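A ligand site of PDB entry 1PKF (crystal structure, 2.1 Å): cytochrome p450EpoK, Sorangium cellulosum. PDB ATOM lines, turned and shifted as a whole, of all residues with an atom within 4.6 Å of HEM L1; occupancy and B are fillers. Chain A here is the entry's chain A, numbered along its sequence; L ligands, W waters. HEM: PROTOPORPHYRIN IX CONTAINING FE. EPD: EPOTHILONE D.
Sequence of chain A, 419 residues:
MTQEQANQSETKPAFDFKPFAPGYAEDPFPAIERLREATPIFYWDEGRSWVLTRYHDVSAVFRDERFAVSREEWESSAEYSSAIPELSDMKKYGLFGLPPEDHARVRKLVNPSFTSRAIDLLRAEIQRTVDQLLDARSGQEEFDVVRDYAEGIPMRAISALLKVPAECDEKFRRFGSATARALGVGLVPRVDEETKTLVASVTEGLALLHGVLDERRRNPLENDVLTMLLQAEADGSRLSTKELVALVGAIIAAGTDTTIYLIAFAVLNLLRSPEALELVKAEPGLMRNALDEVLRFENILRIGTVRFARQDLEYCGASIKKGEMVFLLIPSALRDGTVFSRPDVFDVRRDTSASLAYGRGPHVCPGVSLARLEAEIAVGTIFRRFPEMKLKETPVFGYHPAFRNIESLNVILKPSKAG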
ATOM      1  N   PHE A  62      -9.391 -17.899  14.591  1.00  0.00           N
ATOM      2  CA  PHE A  62     -10.732 -17.298  14.534  1.00  0.00           C
ATOM      3  C   PHE A  62     -10.720 -16.016  13.678  1.00  0.00           C
ATOM      4  O   PHE A  62     -11.613 -15.786  12.855  1.00  0.00           O
ATOM      5  CB  PHE A  62     -11.227 -16.956  15.946  1.00  0.00           C
ATOM      6  CG  PHE A  62     -12.053 -18.042  16.633  1.00  0.00           C
ATOM      7  CD1 PHE A  62     -13.291 -18.409  16.149  1.00  0.00           C
ATOM      8  CD2 PHE A  62     -11.617 -18.597  17.816  1.00  0.00           C
ATOM      9  CE1 PHE A  62     -14.070 -19.378  16.828  1.00  0.00           C
ATOM     10  CE2 PHE A  62     -12.362 -19.548  18.478  1.00  0.00           C
ATOM     11  CZ  PHE A  62     -13.594 -19.955  17.989  1.00  0.00           C
ATOM     12  N   LEU A  95     -25.109 -19.623   7.516  1.00  0.00           N
ATOM     13  CA  LEU A  95     -24.069 -18.723   7.939  1.00  0.00           C
ATOM     14  C   LEU A  95     -22.661 -19.314   7.770  1.00  0.00           C
ATOM     15  O   LEU A  95     -21.692 -18.583   7.577  1.00  0.00           O
ATOM     16  CB  LEU A  95     -24.310 -18.246   9.367  1.00  0.00           C
ATOM     17  CG  LEU A  95     -25.504 -17.272   9.420  1.00  0.00           C
ATOM     18  CD1 LEU A  95     -26.027 -17.074  10.816  1.00  0.00           C
ATOM     19  CD2 LEU A  95     -25.162 -15.928   8.815  1.00  0.00           C
ATOM     20  N   PHE A  96     -22.551 -20.637   7.781  1.00  0.00           N
ATOM     21  CA  PHE A  96     -21.222 -21.242   7.602  1.00  0.00           C
ATOM     22  C   PHE A  96     -20.796 -21.275   6.124  1.00  0.00           C
ATOM     23  O   PHE A  96     -19.612 -21.129   5.822  1.00  0.00           O
ATOM     24  CB  PHE A  96     -21.136 -22.628   8.267  1.00  0.00           C
ATOM     25  CG  PHE A  96     -21.069 -22.568   9.789  1.00  0.00           C
ATOM     26  CD1 PHE A  96     -21.328 -23.697  10.548  1.00  0.00           C
ATOM     27  CD2 PHE A  96     -20.779 -21.376  10.445  1.00  0.00           C
ATOM     28  CE1 PHE A  96     -21.266 -23.671  11.936  1.00  0.00           C
ATOM     29  CE2 PHE A  96     -20.707 -21.337  11.838  1.00  0.00           C
ATOM     30  CZ  PHE A  96     -20.945 -22.472  12.590  1.00  0.00           C
ATOM     31  N   HIS A 103     -21.975 -13.142   4.152  1.00  0.00           N
ATOM     32  CA  HIS A 103     -22.126 -13.466   5.550  1.00  0.00           C
ATOM     33  C   HIS A 103     -22.275 -12.195   6.371  1.00  0.00           C
ATOM     34  O   HIS A 103     -23.107 -12.139   7.261  1.00  0.00           O
ATOM     35  CB  HIS A 103     -20.938 -14.268   6.043  1.00  0.00           C
ATOM     36  CG  HIS A 103     -20.916 -14.453   7.532  1.00  0.00           C
ATOM     37  ND1 HIS A 103     -20.121 -13.699   8.362  1.00  0.00           N
ATOM     38  CD2 HIS A 103     -21.639 -15.270   8.344  1.00  0.00           C
ATOM     39  CE1 HIS A 103     -20.326 -14.062   9.615  1.00  0.00           C
ATOM     40  NE2 HIS A 103     -21.240 -15.013   9.633  1.00  0.00           N
ATOM     41  N   ARG A 107     -25.521 -11.143   8.678  1.00  0.00           N
ATOM     42  CA  ARG A 107     -25.302 -10.790  10.094  1.00  0.00           C
ATOM     43  C   ARG A 107     -25.722  -9.356  10.432  1.00  0.00           C
ATOM     44  O   ARG A 107     -26.344  -9.116  11.444  1.00  0.00           O
ATOM     45  CB  ARG A 107     -23.834 -11.001  10.504  1.00  0.00           C
ATOM     46  CG  ARG A 107     -23.423 -12.457  10.773  1.00  0.00           C
ATOM     47  CD  ARG A 107     -24.248 -13.210  11.797  1.00  0.00           C
ATOM     48  NE  ARG A 107     -24.105 -12.734  13.185  1.00  0.00           N
ATOM     49  CZ  ARG A 107     -23.215 -13.179  14.062  1.00  0.00           C
ATOM     50  NH1 ARG A 107     -22.355 -14.127  13.719  1.00  0.00           N
ATOM     51  NH2 ARG A 107     -23.205 -12.691  15.303  1.00  0.00           N
ATOM     52  N   PHE A 114     -30.801  -9.674  18.190  1.00  0.00           N
ATOM     53  CA  PHE A 114     -30.276 -10.541  19.226  1.00  0.00           C
ATOM     54  C   PHE A 114     -29.519  -9.823  20.361  1.00  0.00           C
ATOM     55  O   PHE A 114     -28.897 -10.473  21.175  1.00  0.00           O
ATOM     56  CB  PHE A 114     -29.385 -11.599  18.587  1.00  0.00           C
ATOM     57  CG  PHE A 114     -30.145 -12.740  17.983  1.00  0.00           C
ATOM     58  CD1 PHE A 114     -30.515 -12.699  16.668  1.00  0.00           C
ATOM     59  CD2 PHE A 114     -30.497 -13.821  18.758  1.00  0.00           C
ATOM     60  CE1 PHE A 114     -31.239 -13.743  16.097  1.00  0.00           C
ATOM     61  CE2 PHE A 114     -31.197 -14.889  18.204  1.00  0.00           C
ATOM     62  CZ  PHE A 114     -31.577 -14.842  16.870  1.00  0.00           C
ATOM     63  N   ILE A 158     -36.652 -19.739  21.754  1.00  0.00           N
ATOM     64  CA  ILE A 158     -36.525 -19.422  20.346  1.00  0.00           C
ATOM     65  C   ILE A 158     -37.914 -19.253  19.684  1.00  0.00           C
ATOM     66  O   ILE A 158     -38.114 -18.358  18.898  1.00  0.00           O
ATOM     67  CB  ILE A 158     -35.703 -20.517  19.631  1.00  0.00           C
ATOM     68  CG1 ILE A 158     -34.222 -20.385  20.001  1.00  0.00           C
ATOM     69  CG2 ILE A 158     -35.842 -20.377  18.131  1.00  0.00           C
ATOM     70  CD1 ILE A 158     -33.356 -21.598  19.577  1.00  0.00           C
ATOM     71  N   ALA A 250     -30.890 -22.446  11.099  1.00  0.00           N
ATOM     72  CA  ALA A 250     -29.619 -22.528  11.822  1.00  0.00           C
ATOM     73  C   ALA A 250     -29.762 -22.015  13.238  1.00  0.00           C
ATOM     74  O   ALA A 250     -29.169 -22.558  14.172  1.00  0.00           O
ATOM     75  CB  ALA A 250     -28.520 -21.735  11.087  1.00  0.00           C
ATOM     76  N   ILE A 251     -30.564 -20.964  13.386  1.00  0.00           N
ATOM     77  CA  ILE A 251     -30.844 -20.405  14.693  1.00  0.00           C
ATOM     78  C   ILE A 251     -31.516 -21.476  15.535  1.00  0.00           C
ATOM     79  O   ILE A 251     -31.143 -21.687  16.686  1.00  0.00           O
ATOM     80  CB  ILE A 251     -31.690 -19.132  14.552  1.00  0.00           C
ATOM     81  CG1 ILE A 251     -30.794 -17.953  14.234  1.00  0.00           C
ATOM     82  CG2 ILE A 251     -32.498 -18.870  15.817  1.00  0.00           C
ATOM     83  CD1 ILE A 251     -31.505 -16.723  13.766  1.00  0.00           C
ATOM     84  N   ALA A 254     -28.704 -24.313  16.071  1.00  0.00           N
ATOM     85  CA  ALA A 254     -27.614 -23.830  16.917  1.00  0.00           C
ATOM     86  C   ALA A 254     -28.063 -23.576  18.360  1.00  0.00           C
ATOM     87  O   ALA A 254     -27.285 -23.736  19.290  1.00  0.00           O
ATOM     88  CB  ALA A 254     -26.988 -22.572  16.328  1.00  0.00           C
ATOM     89  N   GLY A 255     -29.305 -23.185  18.569  1.00  0.00           N
ATOM     90  CA  GLY A 255     -29.728 -22.697  19.869  1.00  0.00           C
ATOM     91  C   GLY A 255     -30.443 -23.660  20.773  1.00  0.00           C
ATOM     92  O   GLY A 255     -30.777 -23.338  21.929  1.00  0.00           O
ATOM     93  N   THR A 258     -27.194 -26.649  22.565  1.00  0.00           N
ATOM     94  CA  THR A 258     -26.160 -25.872  23.265  1.00  0.00           C
ATOM     95  C   THR A 258     -26.680 -25.357  24.587  1.00  0.00           C
ATOM     96  O   THR A 258     -26.052 -25.519  25.607  1.00  0.00           O
ATOM     97  CB  THR A 258     -25.726 -24.673  22.381  1.00  0.00           C
ATOM     98  OG1 THR A 258     -26.870 -23.987  21.850  1.00  0.00           O
ATOM     99  CG2 THR A 258     -25.002 -25.155  21.137  1.00  0.00           C
ATOM    100  N   THR A 259     -27.839 -24.733  24.576  1.00  0.00           N
ATOM    101  CA  THR A 259     -28.365 -24.137  25.775  1.00  0.00           C
ATOM    102  C   THR A 259     -28.826 -25.179  26.758  1.00  0.00           C
ATOM    103  O   THR A 259     -28.759 -24.949  27.963  1.00  0.00           O
ATOM    104  CB  THR A 259     -29.524 -23.221  25.411  1.00  0.00           C
ATOM    105  OG1 THR A 259     -29.093 -22.315  24.412  1.00  0.00           O
ATOM    106  CG2 THR A 259     -29.921 -22.341  26.602  1.00  0.00           C
ATOM    107  N   LEU A 262     -25.630 -25.975  28.532  1.00  0.00           N
ATOM    108  CA  LEU A 262     -25.226 -24.877  29.424  1.00  0.00           C
ATOM    109  C   LEU A 262     -25.965 -24.934  30.748  1.00  0.00           C
ATOM    110  O   LEU A 262     -25.353 -24.970  31.826  1.00  0.00           O
ATOM    111  CB  LEU A 262     -25.485 -23.519  28.756  1.00  0.00           C
ATOM    112  CG  LEU A 262     -25.353 -22.286  29.662  1.00  0.00           C
ATOM    113  CD1 LEU A 262     -23.935 -22.202  30.273  1.00  0.00           C
ATOM    114  CD2 LEU A 262     -25.678 -21.062  28.871  1.00  0.00           C
ATOM    115  N   LEU A 295     -18.749 -22.242  31.159  1.00  0.00           N
ATOM    116  CA  LEU A 295     -18.337 -22.530  29.791  1.00  0.00           C
ATOM    117  C   LEU A 295     -16.810 -22.442  29.628  1.00  0.00           C
ATOM    118  O   LEU A 295     -16.200 -23.079  28.754  1.00  0.00           O
ATOM    119  CB  LEU A 295     -19.011 -21.539  28.865  1.00  0.00           C
ATOM    120  CG  LEU A 295     -20.200 -21.916  28.004  1.00  0.00           C
ATOM    121  CD1 LEU A 295     -20.936 -23.208  28.424  1.00  0.00           C
ATOM    122  CD2 LEU A 295     -21.138 -20.770  27.892  1.00  0.00           C
ATOM    123  N   ILE A 300     -18.808 -27.133  26.943  1.00  0.00           N
ATOM    124  CA  ILE A 300     -19.696 -28.182  26.480  1.00  0.00           C
ATOM    125  C   ILE A 300     -19.232 -28.855  25.200  1.00  0.00           C
ATOM    126  O   ILE A 300     -19.785 -29.886  24.821  1.00  0.00           O
ATOM    127  CB  ILE A 300     -21.145 -27.625  26.278  1.00  0.00           C
ATOM    128  CG1 ILE A 300     -21.175 -26.529  25.223  1.00  0.00           C
ATOM    129  CG2 ILE A 300     -21.713 -27.175  27.609  1.00  0.00           C
ATOM    130  CD1 ILE A 300     -22.593 -26.097  24.794  1.00  0.00           C
ATOM    131  N   THR A 305     -14.503 -26.241  17.158  1.00  0.00           N
ATOM    132  CA  THR A 305     -15.108 -25.833  15.916  1.00  0.00           C
ATOM    133  C   THR A 305     -14.055 -25.968  14.848  1.00  0.00           C
ATOM    134  O   THR A 305     -12.911 -26.309  15.158  1.00  0.00           O
ATOM    135  CB  THR A 305     -15.718 -24.418  16.038  1.00  0.00           C
ATOM    136  OG1 THR A 305     -16.397 -24.080  14.817  1.00  0.00           O
ATOM    137  CG2 THR A 305     -14.605 -23.374  16.219  1.00  0.00           C
ATOM    138  N   VAL A 306     -14.424 -25.765  13.599  1.00  0.00           N
ATOM    139  CA  VAL A 306     -13.556 -26.060  12.480  1.00  0.00           C
ATOM    140  C   VAL A 306     -13.298 -24.849  11.585  1.00  0.00           C
ATOM    141  O   VAL A 306     -14.134 -23.946  11.470  1.00  0.00           O
ATOM    142  CB  VAL A 306     -14.110 -27.201  11.578  1.00  0.00           C
ATOM    143  CG1 VAL A 306     -14.113 -28.465  12.363  1.00  0.00           C
ATOM    144  CG2 VAL A 306     -15.528 -26.920  11.092  1.00  0.00           C
ATOM    145  N   ARG A 307     -12.134 -24.883  10.955  1.00  0.00           N
ATOM    146  CA  ARG A 307     -11.788 -23.975   9.890  1.00  0.00           C
ATOM    147  C   ARG A 307     -11.084 -24.801   8.820  1.00  0.00           C
ATOM    148  O   ARG A 307     -10.671 -25.954   9.083  1.00  0.00           O
ATOM    149  CB  ARG A 307     -10.883 -22.853  10.408  1.00  0.00           C
ATOM    150  CG  ARG A 307     -11.555 -21.929  11.425  1.00  0.00           C
ATOM    151  CD  ARG A 307     -12.625 -21.085  10.791  1.00  0.00           C
ATOM    152  NE  ARG A 307     -13.183 -20.019  11.637  1.00  0.00           N
ATOM    153  CZ  ARG A 307     -14.189 -20.193  12.487  1.00  0.00           C
ATOM    154  NH1 ARG A 307     -14.679 -21.416  12.689  1.00  0.00           N
ATOM    155  NH2 ARG A 307     -14.650 -19.155  13.181  1.00  0.00           N
ATOM    156  N   ALA A 357     -15.680 -19.131  24.427  1.00  0.00           N
ATOM    157  CA  ALA A 357     -16.769 -20.087  24.350  1.00  0.00           C
ATOM    158  C   ALA A 357     -17.842 -19.692  23.358  1.00  0.00           C
ATOM    159  O   ALA A 357     -18.490 -20.555  22.831  1.00  0.00           O
ATOM    160  CB  ALA A 357     -17.383 -20.333  25.727  1.00  0.00           C
ATOM    161  N   TYR A 358     -18.002 -18.396  23.089  1.00  0.00           N
ATOM    162  CA  TYR A 358     -18.982 -17.910  22.130  1.00  0.00           C
ATOM    163  C   TYR A 358     -18.355 -17.465  20.840  1.00  0.00           C
ATOM    164  O   TYR A 358     -19.006 -16.824  20.006  1.00  0.00           O
ATOM    165  CB  TYR A 358     -19.830 -16.813  22.712  1.00  0.00           C
ATOM    166  CG  TYR A 358     -20.750 -17.296  23.796  1.00  0.00           C
ATOM    167  CD1 TYR A 358     -20.440 -17.124  25.115  1.00  0.00           C
ATOM    168  CD2 TYR A 358     -21.937 -17.946  23.480  1.00  0.00           C
ATOM    169  CE1 TYR A 358     -21.281 -17.551  26.103  1.00  0.00           C
ATOM    170  CE2 TYR A 358     -22.785 -18.397  24.465  1.00  0.00           C
ATOM    171  CZ  TYR A 358     -22.445 -18.205  25.789  1.00  0.00           C
ATOM    172  OH  TYR A 358     -23.288 -18.643  26.791  1.00  0.00           O
ATOM    173  N   GLY A 359     -17.106 -17.833  20.635  1.00  0.00           N
ATOM    174  CA  GLY A 359     -16.449 -17.457  19.401  1.00  0.00           C
ATOM    175  C   GLY A 359     -15.740 -16.102  19.415  1.00  0.00           C
ATOM    176  O   GLY A 359     -15.743 -15.380  20.397  1.00  0.00           O
ATOM    177  N   PRO A 362     -16.117 -12.338  12.899  1.00  0.00           N
ATOM    178  CA  PRO A 362     -17.405 -12.257  12.216  1.00  0.00           C
ATOM    179  C   PRO A 362     -18.421 -13.372  12.578  1.00  0.00           C
ATOM    180  O   PRO A 362     -19.619 -13.104  12.434  1.00  0.00           O
ATOM    181  CB  PRO A 362     -17.021 -12.343  10.742  1.00  0.00           C
ATOM    182  CG  PRO A 362     -15.651 -11.727  10.689  1.00  0.00           C
ATOM    183  CD  PRO A 362     -14.988 -12.295  11.951  1.00  0.00           C
ATOM    184  N   HIS A 363     -17.967 -14.537  13.057  1.00  0.00           N
ATOM    185  CA  HIS A 363     -18.890 -15.661  13.266  1.00  0.00           C
ATOM    186  C   HIS A 363     -19.243 -15.817  14.731  1.00  0.00           C
ATOM    187  O   HIS A 363     -19.828 -16.818  15.144  1.00  0.00           O
ATOM    188  CB  HIS A 363     -18.325 -16.950  12.700  1.00  0.00           C
ATOM    189  CG  HIS A 363     -18.343 -17.025  11.206  1.00  0.00           C
ATOM    190  ND1 HIS A 363     -19.411 -17.531  10.499  1.00  0.00           N
ATOM    191  CD2 HIS A 363     -17.419 -16.661  10.296  1.00  0.00           C
ATOM    192  CE1 HIS A 363     -19.136 -17.486   9.206  1.00  0.00           C
ATOM    193  NE2 HIS A 363     -17.943 -16.948   9.062  1.00  0.00           N
ATOM    194  N   VAL A 364     -18.903 -14.790  15.487  1.00  0.00           N
ATOM    195  CA  VAL A 364     -19.198 -14.746  16.912  1.00  0.00           C
ATOM    196  C   VAL A 364     -20.687 -15.020  17.086  1.00  0.00           C
ATOM    197  O   VAL A 364     -21.511 -14.544  16.352  1.00  0.00           O
ATOM    198  CB  VAL A 364     -18.797 -13.372  17.512  1.00  0.00           C
ATOM    199  CG1 VAL A 364     -19.559 -12.220  16.806  1.00  0.00           C
ATOM    200  CG2 VAL A 364     -19.034 -13.325  19.023  1.00  0.00           C
ATOM    201  N   CYS A 365     -20.990 -15.829  18.072  1.00  0.00           N
ATOM    202  CA  CYS A 365     -22.317 -16.325  18.292  1.00  0.00           C
ATOM    203  C   CYS A 365     -23.323 -15.195  18.449  1.00  0.00           C
ATOM    204  O   CYS A 365     -23.193 -14.370  19.359  1.00  0.00           O
ATOM    205  CB  CYS A 365     -22.323 -17.162  19.560  1.00  0.00           C
ATOM    206  SG  CYS A 365     -23.967 -17.808  20.020  1.00  0.00           S
ATOM    207  N   PRO A 366     -24.345 -15.180  17.599  1.00  0.00           N
ATOM    208  CA  PRO A 366     -25.412 -14.194  17.742  1.00  0.00           C
ATOM    209  C   PRO A 366     -26.293 -14.491  18.917  1.00  0.00           C
ATOM    210  O   PRO A 366     -26.809 -13.573  19.492  1.00  0.00           O
ATOM    211  CB  PRO A 366     -26.160 -14.272  16.390  1.00  0.00           C
ATOM    212  CG  PRO A 366     -25.860 -15.708  15.826  1.00  0.00           C
ATOM    213  CD  PRO A 366     -24.524 -16.054  16.423  1.00  0.00           C
ATOM    214  N   GLY A 367     -26.381 -15.737  19.360  1.00  0.00           N
ATOM    215  CA  GLY A 367     -27.281 -16.059  20.427  1.00  0.00           C
ATOM    216  C   GLY A 367     -26.769 -15.936  21.850  1.00  0.00           C
ATOM    217  O   GLY A 367     -27.468 -16.372  22.775  1.00  0.00           O
ATOM    218  N   ALA A 371     -28.753 -17.035  25.203  1.00  0.00           N
ATOM    219  CA  ALA A 371     -28.303 -18.161  26.003  1.00  0.00           C
ATOM    220  C   ALA A 371     -28.110 -17.740  27.448  1.00  0.00           C
ATOM    221  O   ALA A 371     -28.517 -18.461  28.347  1.00  0.00           O
ATOM    222  CB  ALA A 371     -26.987 -18.718  25.460  1.00  0.00           C
ATOM    223  N   GLU A 374     -31.645 -17.089  29.203  1.00  0.00           N
ATOM    224  CA  GLU A 374     -32.312 -18.351  29.515  1.00  0.00           C
ATOM    225  C   GLU A 374     -31.665 -19.045  30.698  1.00  0.00           C
ATOM    226  O   GLU A 374     -32.341 -19.539  31.592  1.00  0.00           O
ATOM    227  CB  GLU A 374     -32.255 -19.317  28.319  1.00  0.00           C
ATOM    228  CG  GLU A 374     -32.955 -18.843  27.047  1.00  0.00           C
ATOM    229  CD  GLU A 374     -32.815 -19.872  25.930  1.00  0.00           C
ATOM    230  OE1 GLU A 374     -33.129 -21.040  26.206  1.00  0.00           O
ATOM    231  OE2 GLU A 374     -32.382 -19.538  24.824  1.00  0.00           O
HETATM  232  CHA HEM L   1     -22.074 -19.515  16.219  1.00  0.00           C
HETATM  233  CHB HEM L   1     -21.327 -21.073  20.620  1.00  0.00           C
HETATM  234  CHC HEM L   1     -26.010 -20.614  21.812  1.00  0.00           C
HETATM  235  CHD HEM L   1     -26.814 -19.382  17.333  1.00  0.00           C
HETATM  236  C1A HEM L   1     -21.455 -19.887  17.361  1.00  0.00           C
HETATM  237  C2A HEM L   1     -20.028 -20.071  17.509  1.00  0.00           C
HETATM  238  C3A HEM L   1     -19.825 -20.520  18.729  1.00  0.00           C
HETATM  239  C4A HEM L   1     -21.102 -20.631  19.377  1.00  0.00           C
HETATM  240  CMA HEM L   1     -18.440 -20.834  19.300  1.00  0.00           C
HETATM  241  CAA HEM L   1     -18.962 -19.796  16.441  1.00  0.00           C
HETATM  242  CBA HEM L   1     -18.541 -21.132  15.799  1.00  0.00           C
HETATM  243  CGA HEM L   1     -17.442 -20.873  14.799  1.00  0.00           C
HETATM  244  O1A HEM L   1     -17.062 -21.813  14.051  1.00  0.00           O
HETATM  245  O2A HEM L   1     -16.928 -19.715  14.720  1.00  0.00           O
HETATM  246  C1B HEM L   1     -22.542 -21.097  21.227  1.00  0.00           C
HETATM  247  C2B HEM L   1     -22.713 -21.555  22.583  1.00  0.00           C
HETATM  248  C3B HEM L   1     -23.986 -21.372  22.888  1.00  0.00           C
HETATM  249  C4B HEM L   1     -24.658 -20.880  21.743  1.00  0.00           C
HETATM  250  CMB HEM L   1     -21.633 -22.103  23.581  1.00  0.00           C
HETATM  251  CAB HEM L   1     -24.710 -21.752  24.171  1.00  0.00           C
HETATM  252  CBB HEM L   1     -24.245 -21.444  25.358  1.00  0.00           C
HETATM  253  C1C HEM L   1     -26.686 -20.178  20.756  1.00  0.00           C
HETATM  254  C2C HEM L   1     -28.079 -19.781  20.673  1.00  0.00           C
HETATM  255  C3C HEM L   1     -28.294 -19.442  19.414  1.00  0.00           C
HETATM  256  C4C HEM L   1     -27.029 -19.563  18.663  1.00  0.00           C
HETATM  257  CMC HEM L   1     -29.116 -19.793  21.797  1.00  0.00           C
HETATM  258  CAC HEM L   1     -29.646 -18.999  18.913  1.00  0.00           C
HETATM  259  CBC HEM L   1     -29.697 -18.352  17.791  1.00  0.00           C
HETATM  260  C1D HEM L   1     -25.629 -19.414  16.651  1.00  0.00           C
HETATM  261  C2D HEM L   1     -25.562 -19.210  15.222  1.00  0.00           C
HETATM  262  C3D HEM L   1     -24.097 -19.239  14.878  1.00  0.00           C
HETATM  263  C4D HEM L   1     -23.440 -19.476  16.130  1.00  0.00           C
HETATM  264  CMD HEM L   1     -26.672 -18.943  14.204  1.00  0.00           C
HETATM  265  CAD HEM L   1     -23.481 -19.033  13.508  1.00  0.00           C
HETATM  266  CBD HEM L   1     -22.926 -17.615  13.537  1.00  0.00           C
HETATM  267  CGD HEM L   1     -22.190 -17.315  12.265  1.00  0.00           C
HETATM  268  O1D HEM L   1     -21.615 -18.231  11.644  1.00  0.00           O
HETATM  269  O2D HEM L   1     -22.167 -16.149  11.830  1.00  0.00           O
HETATM  270  NA  HEM L   1     -22.082 -20.251  18.515  1.00  0.00           N
HETATM  271  NB  HEM L   1     -23.774 -20.686  20.675  1.00  0.00           N
HETATM  272  NC  HEM L   1     -26.102 -20.008  19.547  1.00  0.00           N
HETATM  273  ND  HEM L   1     -24.347 -19.571  17.199  1.00  0.00           N
HETATM  274 FE   HEM L   1     -24.069 -19.937  19.126  1.00  0.00          FE
HETATM  275  C51 EPD L   2     -21.922 -24.349  19.729  1.00  0.00           C
HETATM  276  C5  EPD L   2     -21.995 -24.338  18.207  1.00  0.00           C
HETATM  277  C4  EPD L   2     -23.221 -24.307  17.717  1.00  0.00           C
HETATM  278  C3  EPD L   2     -23.497 -24.075  16.262  1.00  0.00           C
HETATM  279  C2  EPD L   2     -24.357 -25.223  15.655  1.00  0.00           C
HETATM  280  C20 EPD L   2     -24.703 -24.998  14.109  1.00  0.00           C
HETATM  281  C21 EPD L   2     -25.170 -26.229  13.333  1.00  0.00           C
HETATM  282  C22 EPD L   2     -24.484 -23.761  13.628  1.00  0.00           C
HETATM  283  C23 EPD L   2     -24.706 -23.380  12.276  1.00  0.00           C
HETATM  284  C24 EPD L   2     -24.700 -22.233  11.688  1.00  0.00           C
HETATM  285  S1  EPD L   2     -24.994 -22.352   9.972  1.00  0.00           S
HETATM  286  C25 EPD L   2     -25.085 -24.055  10.211  1.00  0.00           C
HETATM  287  C27 EPD L   2     -25.368 -24.898   8.993  1.00  0.00           C
HETATM  288  N26 EPD L   2     -24.914 -24.477  11.373  1.00  0.00           N
HETATM  289  C6  EPD L   2     -20.802 -23.840  17.373  1.00  0.00           C
HETATM  290  C7  EPD L   2     -19.498 -24.577  17.656  1.00  0.00           C
HETATM  291  C8  EPD L   2     -19.584 -25.981  17.017  1.00  0.00           C
HETATM  292  C9  EPD L   2     -18.970 -26.425  15.721  1.00  0.00           C
HETATM  293  C91 EPD L   2     -19.474 -25.975  14.399  1.00  0.00           C
HETATM  294  C10 EPD L   2     -19.461 -27.953  15.776  1.00  0.00           C
HETATM  295  O10 EPD L   2     -18.840 -28.527  16.990  1.00  0.00           O
HETATM  296  C11 EPD L   2     -19.291 -28.795  14.447  1.00  0.00           C
HETATM  297  C28 EPD L   2     -17.844 -29.015  14.006  1.00  0.00           C
HETATM  298  C12 EPD L   2     -19.966 -30.161  14.553  1.00  0.00           C
HETATM  299  O12 EPD L   2     -19.341 -30.990  15.226  1.00  0.00           O
HETATM  300  C13 EPD L   2     -21.332 -30.324  13.839  1.00  0.00           C
HETATM  301  C30 EPD L   2     -21.278 -30.098  12.345  1.00  0.00           C
HETATM  302  C29 EPD L   2     -22.021 -31.640  14.202  1.00  0.00           C
HETATM  303  C14 EPD L   2     -22.312 -29.148  14.315  1.00  0.00           C
HETATM  304  O14 EPD L   2     -23.522 -29.063  13.557  1.00  0.00           O
HETATM  305  C15 EPD L   2     -22.849 -29.246  15.720  1.00  0.00           C
HETATM  306  C16 EPD L   2     -23.670 -27.963  16.081  1.00  0.00           C
HETATM  307  O16 EPD L   2     -24.414 -27.990  17.051  1.00  0.00           O
HETATM  308  O1  EPD L   2     -23.546 -26.748  15.291  1.00  0.00           O
HETATM  309  O   HOH W   1     -16.627 -17.398  16.176  1.00  0.00           O
HETATM  310  O   HOH W   2     -17.048 -23.733  11.741  1.00  0.00           O
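Water W1 lies within hydrogen-bond range of O2A of HEM L1 (2.8 Å) and O of His 363 (3.4 Å).
Water W2 lies within hydrogen-bond range of the backbone carbonyl oxygen of Val 306 (2.9 Å), an oxygen (O1A) of HEM L1 (3.0 Å), the side-chain hydroxyl of Thr 305 (3.2 Å) and the guanidinium group of Arg 307 (3.4 Å).
An iron atom (FE) of HEM L1 is bound by the side-chain sulfur (SG) of Cys 365 (2.3 Å).
The side-chain hydroxyl (OG1) of Thr 305 sits at hydrogen-bond distance from an oxygen (O1A) of HEM L1.
A ring nitrogen (ND1) of His 363 sits at hydrogen-bond distance from an oxygen (O1D) of HEM L1, at 2.6 Å.
An oxygen (O2D) of HEM L1 is in hydrogen-bond range of a ring nitrogen (NE2) of His 103.
O2D of HEM L1 is in salt-bridge range of NH1 of Arg 107.
The guanidinium group (NH1) of Arg 307 lies within salt-bridge range of an oxygen (O1A) of HEM L1.
The backbone NH (N) of Phe 96 sits close to a sulfur (S1) of EPD L2.
S1 of EPD L2 lies close to N of Leu 95 (3.7 Å).
Phe 62 touches HEM L1.
CB of Leu 95 touches O1D of HEM L1 (3.5 Å).
Phe 96 touches HEM L1.
Phe 114 touches HEM L1 (CE2 to CBC, 3.8 Å).
CG2 of Ile 251 touches CBC of HEM L1, 3.5 Å away.
CB of Ala 254 touches CHD of HEM L1, at 3.3 Å.
Gly 255 touches HEM L1.
OG1 of Thr 258 touches CHC of HEM L1, 3.5 Å away.
Thr 259 touches HEM L1 (OG1 to CMC, 3.6 Å).
CD2 of Leu 262 touches CBB of HEM L1, at 3.8 Å.
Ala 357 touches HEM L1.
OH of Tyr 358 touches CBB of HEM L1, 3.3 Å away.
Gly 359 touches HEM L1.
CD of Pro 366 touches C2D of HEM L1, 3.5 Å away.
CA of Gly 367 touches C3C of HEM L1, at 3.7 Å.
Ala 371 touches HEM L1.
Hydrophobic or aromatic side chains within 4 Å of HEM L1: Phe 62, Leu 95, Phe 96, His 103, Phe 114, Ile 251, Ala 254, Leu 262, Tyr 358, His 363, Pro 366 and Ala 371.
Of the 30 residues printed, 22 come within 4 Å of HEM L1.
The nearest printed residue that does not touch HEM L1 is Pro 362 (4.02 Å).
The backbone carbonyl oxygen (O) of Tyr 358 is in hydrogen-bond range of the backbone NH (N) of Cys 365.
N of Gly 367 sits close to SG of Cys 365, 3.2 Å away.
A ring nitrogen (ND1) of His 363 is in hydrogen-bond range of a ring nitrogen (NE2) of His 103.
O of Pro 362 is in hydrogen-bond range of NH1 of Arg 107, at 3.2 Å.
NH2 of Arg 107 sits at hydrogen-bond distance from O of Val 364 (2.7 Å).
The backbone carbonyl oxygen (O) of Ala 254 is in hydrogen-bond range of the side-chain hydroxyl (OG1) of Thr 258, 2.6 Å away.
O of Gly 255 is in hydrogen-bond range of OG1 of Thr 259, 3.2 Å away.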
